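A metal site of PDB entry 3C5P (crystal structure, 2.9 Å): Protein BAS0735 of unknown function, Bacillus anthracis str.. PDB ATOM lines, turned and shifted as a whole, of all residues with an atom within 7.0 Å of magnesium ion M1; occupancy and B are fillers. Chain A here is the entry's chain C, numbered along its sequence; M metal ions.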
ATOM      1  N   PRO A 129      13.056  -7.344  16.518  1.00  0.00           N
ATOM      2  CA  PRO A 129      11.753  -7.325  17.155  1.00  0.00           C
ATOM      3  C   PRO A 129      10.609  -7.090  16.164  1.00  0.00           C
ATOM      4  O   PRO A 129      10.839  -6.551  15.078  1.00  0.00           O
ATOM      5  CB  PRO A 129      11.881  -6.172  18.147  1.00  0.00           C
ATOM      6  CG  PRO A 129      12.881  -5.268  17.540  1.00  0.00           C
ATOM      7  CD  PRO A 129      13.825  -6.114  16.777  1.00  0.00           C
ATOM      8  N   ASP A 131       7.358  -5.042  15.247  1.00  0.00           N
ATOM      9  CA  ASP A 131       7.015  -3.690  15.604  1.00  0.00           C
ATOM     10  C   ASP A 131       5.713  -3.315  14.956  1.00  0.00           C
ATOM     11  O   ASP A 131       5.463  -3.716  13.815  1.00  0.00           O
ATOM     12  CB  ASP A 131       8.046  -2.706  15.047  1.00  0.00           C
ATOM     13  CG  ASP A 131       9.354  -2.760  15.772  1.00  0.00           C
ATOM     14  OD1 ASP A 131       9.386  -2.439  16.983  1.00  0.00           O
ATOM     15  OD2 ASP A 131      10.381  -3.083  15.125  1.00  0.00           O
ATOM     16  N   HIS A 150       3.384  -1.367  10.235  1.00  0.00           N
ATOM     17  CA  HIS A 150       3.892  -2.600  10.865  1.00  0.00           C
ATOM     18  C   HIS A 150       4.965  -3.305  10.023  1.00  0.00           C
ATOM     19  O   HIS A 150       5.054  -3.041   8.806  1.00  0.00           O
ATOM     20  CB  HIS A 150       2.741  -3.549  11.138  1.00  0.00           C
ATOM     21  CG  HIS A 150       1.941  -3.870   9.918  1.00  0.00           C
ATOM     22  ND1 HIS A 150       2.188  -4.992   9.154  1.00  0.00           N
ATOM     23  CD2 HIS A 150       0.907  -3.229   9.332  1.00  0.00           C
ATOM     24  CE1 HIS A 150       1.330  -5.022   8.150  1.00  0.00           C
ATOM     25  NE2 HIS A 150       0.537  -3.969   8.242  1.00  0.00           N
ATOM     26  N   ASP A 151       5.782  -4.144  10.668  1.00  0.00           N
ATOM     27  CA  ASP A 151       6.705  -5.057   9.971  1.00  0.00           C
ATOM     28  C   ASP A 151       5.885  -6.017   9.097  1.00  0.00           C
ATOM     29  O   ASP A 151       4.706  -6.258   9.355  1.00  0.00           O
ATOM     30  CB  ASP A 151       7.531  -5.880  10.977  1.00  0.00           C
ATOM     31  CG  ASP A 151       8.642  -5.066  11.687  1.00  0.00           C
ATOM     32  OD1 ASP A 151       9.297  -4.128  11.164  1.00  0.00           O
ATOM     33  OD2 ASP A 151       8.937  -5.424  12.838  1.00  0.00           O
ATOM     34  N   GLY A 152       6.491  -6.566   8.037  1.00  0.00           N
ATOM     35  CA  GLY A 152       5.740  -7.461   7.136  1.00  0.00           C
ATOM     36  C   GLY A 152       5.526  -8.888   7.615  1.00  0.00           C
ATOM     37  O   GLY A 152       5.116  -9.757   6.830  1.00  0.00           O
ATOM     38  N   PHE A 153       5.792  -9.144   8.895  1.00  0.00           N
ATOM     39  CA  PHE A 153       5.697 -10.486   9.453  1.00  0.00           C
ATOM     40  C   PHE A 153       5.576 -10.372  10.989  1.00  0.00           C
ATOM     41  O   PHE A 153       6.177  -9.482  11.565  1.00  0.00           O
ATOM     42  CB  PHE A 153       6.966 -11.266   9.087  1.00  0.00           C
ATOM     43  CG  PHE A 153       7.040 -12.631   9.708  1.00  0.00           C
ATOM     44  CD1 PHE A 153       6.513 -13.756   9.033  1.00  0.00           C
ATOM     45  CD2 PHE A 153       7.632 -12.800  10.972  1.00  0.00           C
ATOM     46  CE1 PHE A 153       6.565 -15.044   9.606  1.00  0.00           C
ATOM     47  CE2 PHE A 153       7.688 -14.084  11.562  1.00  0.00           C
ATOM     48  CZ  PHE A 153       7.157 -15.204  10.875  1.00  0.00           C
ATOM     49  N   ALA A 183      12.162 -12.306   7.689  1.00  0.00           N
ATOM     50  CA  ALA A 183      13.146 -11.273   7.388  1.00  0.00           C
ATOM     51  C   ALA A 183      12.520  -9.901   7.574  1.00  0.00           C
ATOM     52  O   ALA A 183      13.209  -8.930   7.913  1.00  0.00           O
ATOM     53  CB  ALA A 183      13.681 -11.428   5.961  1.00  0.00           C
ATOM     54  N   ALA A 184      11.205  -9.831   7.369  1.00  0.00           N
ATOM     55  CA  ALA A 184      10.485  -8.573   7.399  1.00  0.00           C
ATOM     56  C   ALA A 184      10.441  -8.007   8.803  1.00  0.00           C
ATOM     57  O   ALA A 184      10.165  -6.828   9.003  1.00  0.00           O
ATOM     58  CB  ALA A 184       9.089  -8.745   6.845  1.00  0.00           C
ATOM     59  N   LEU A 185      10.740  -8.864   9.785  1.00  0.00           N
ATOM     60  CA  LEU A 185      10.910  -8.427  11.156  1.00  0.00           C
ATOM     61  C   LEU A 185      11.957  -7.334  11.299  1.00  0.00           C
ATOM     62  O   LEU A 185      11.842  -6.514  12.208  1.00  0.00           O
ATOM     63  CB  LEU A 185      11.327  -9.605  12.020  1.00  0.00           C
ATOM     64  CG  LEU A 185      10.362 -10.153  13.075  1.00  0.00           C
ATOM     65  CD1 LEU A 185       8.909  -9.806  12.797  1.00  0.00           C
ATOM     66  CD2 LEU A 185      10.531 -11.662  13.209  1.00  0.00           C
ATOM     67  N   GLY A 186      12.956  -7.347  10.420  1.00  0.00           N
ATOM     68  CA  GLY A 186      14.117  -6.507  10.557  1.00  0.00           C
ATOM     69  C   GLY A 186      14.026  -5.232   9.748  1.00  0.00           C
ATOM     70  O   GLY A 186      13.132  -5.067   8.932  1.00  0.00           O
ATOM     71  N   GLY A 187      14.974  -4.320   9.989  1.00  0.00           N
ATOM     72  CA  GLY A 187      15.055  -3.065   9.259  1.00  0.00           C
ATOM     73  C   GLY A 187      13.928  -2.166   9.711  1.00  0.00           C
ATOM     74  O   GLY A 187      13.735  -1.953  10.910  1.00  0.00           O
ATOM     75  N   ASN A 188      13.173  -1.655   8.744  1.00  0.00           N
ATOM     76  CA  ASN A 188      12.102  -0.707   9.037  1.00  0.00           C
ATOM     77  C   ASN A 188      10.710  -1.312   9.124  1.00  0.00           C
ATOM     78  O   ASN A 188      10.537  -2.502   8.844  1.00  0.00           O
ATOM     79  CB  ASN A 188      12.142   0.356   7.959  1.00  0.00           C
ATOM     80  CG  ASN A 188      13.193   1.366   8.226  1.00  0.00           C
ATOM     81  OD1 ASN A 188      13.505   1.641   9.387  1.00  0.00           O
ATOM     82  ND2 ASN A 188      13.767   1.922   7.161  1.00  0.00           N
ATOM     83  N   MET A 189       9.729  -0.501   9.512  1.00  0.00           N
ATOM     84  CA  MET A 189       8.336  -0.916   9.368  1.00  0.00           C
ATOM     85  C   MET A 189       7.884  -0.734   7.924  1.00  0.00           C
ATOM     86  O   MET A 189       7.620   0.373   7.447  1.00  0.00           O
ATOM     87  CB  MET A 189       7.431  -0.215  10.345  1.00  0.00           C
ATOM     88  CG  MET A 189       7.429  -0.882  11.677  1.00  0.00           C
ATOM     89  SD  MET A 189       6.352   0.130  12.942  1.00  0.00           S
ATOM     90  CE  MET A 189       7.470   1.745  13.246  1.00  0.00           C
ATOM     91  N   ASP A 190       7.789  -1.867   7.245  1.00  0.00           N
ATOM     92  CA  ASP A 190       7.705  -1.919   5.815  1.00  0.00           C
ATOM     93  C   ASP A 190       6.291  -1.866   5.206  1.00  0.00           C
ATOM     94  O   ASP A 190       6.157  -1.981   4.008  1.00  0.00           O
ATOM     95  CB  ASP A 190       8.546  -3.123   5.283  1.00  0.00           C
ATOM     96  CG  ASP A 190       8.345  -4.471   6.109  1.00  0.00           C
ATOM     97  OD1 ASP A 190       8.530  -4.532   7.357  1.00  0.00           O
ATOM     98  OD2 ASP A 190       8.075  -5.508   5.469  1.00  0.00           O
HETATM   99 MG    MG M   1      10.867  -4.716   9.087  1.00  0.00          MG
HETATM  100 MG    MG M   2      11.107  -4.794  13.885  1.00  0.00          MG
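The side-chain carboxylate (OD1) of Asp 190 lies within hydrogen-bond range of the backbone NH (N) of Gly 152 (3.0 Å).
N of Asp 190 sits at hydrogen-bond distance from O of His 150 (3.4 Å).
Leu 185 touches magnesium ion M1.
Asp 190 touches magnesium ion M1 (OD1 to MG, 2.9 Å).
Six residues have an atom within 4 Å of magnesium ion M1: Asp 151, Ala 184, Leu 185, Gly 186, Asn 188 and Asp 190.
Magnesium ion M1 is bound by the backbone carbonyl oxygen (O) of Ala 184 (2.2 Å).
Magnesium ion M1 is bound by the backbone carbonyl oxygen (O) of Asn 188 (2.3 Å).
O of Gly 186 is bound to magnesium ion M1 (2.3 Å).
Slightly farther from magnesium ion M1 lies OD1 of Asp 151 (2.7 Å).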
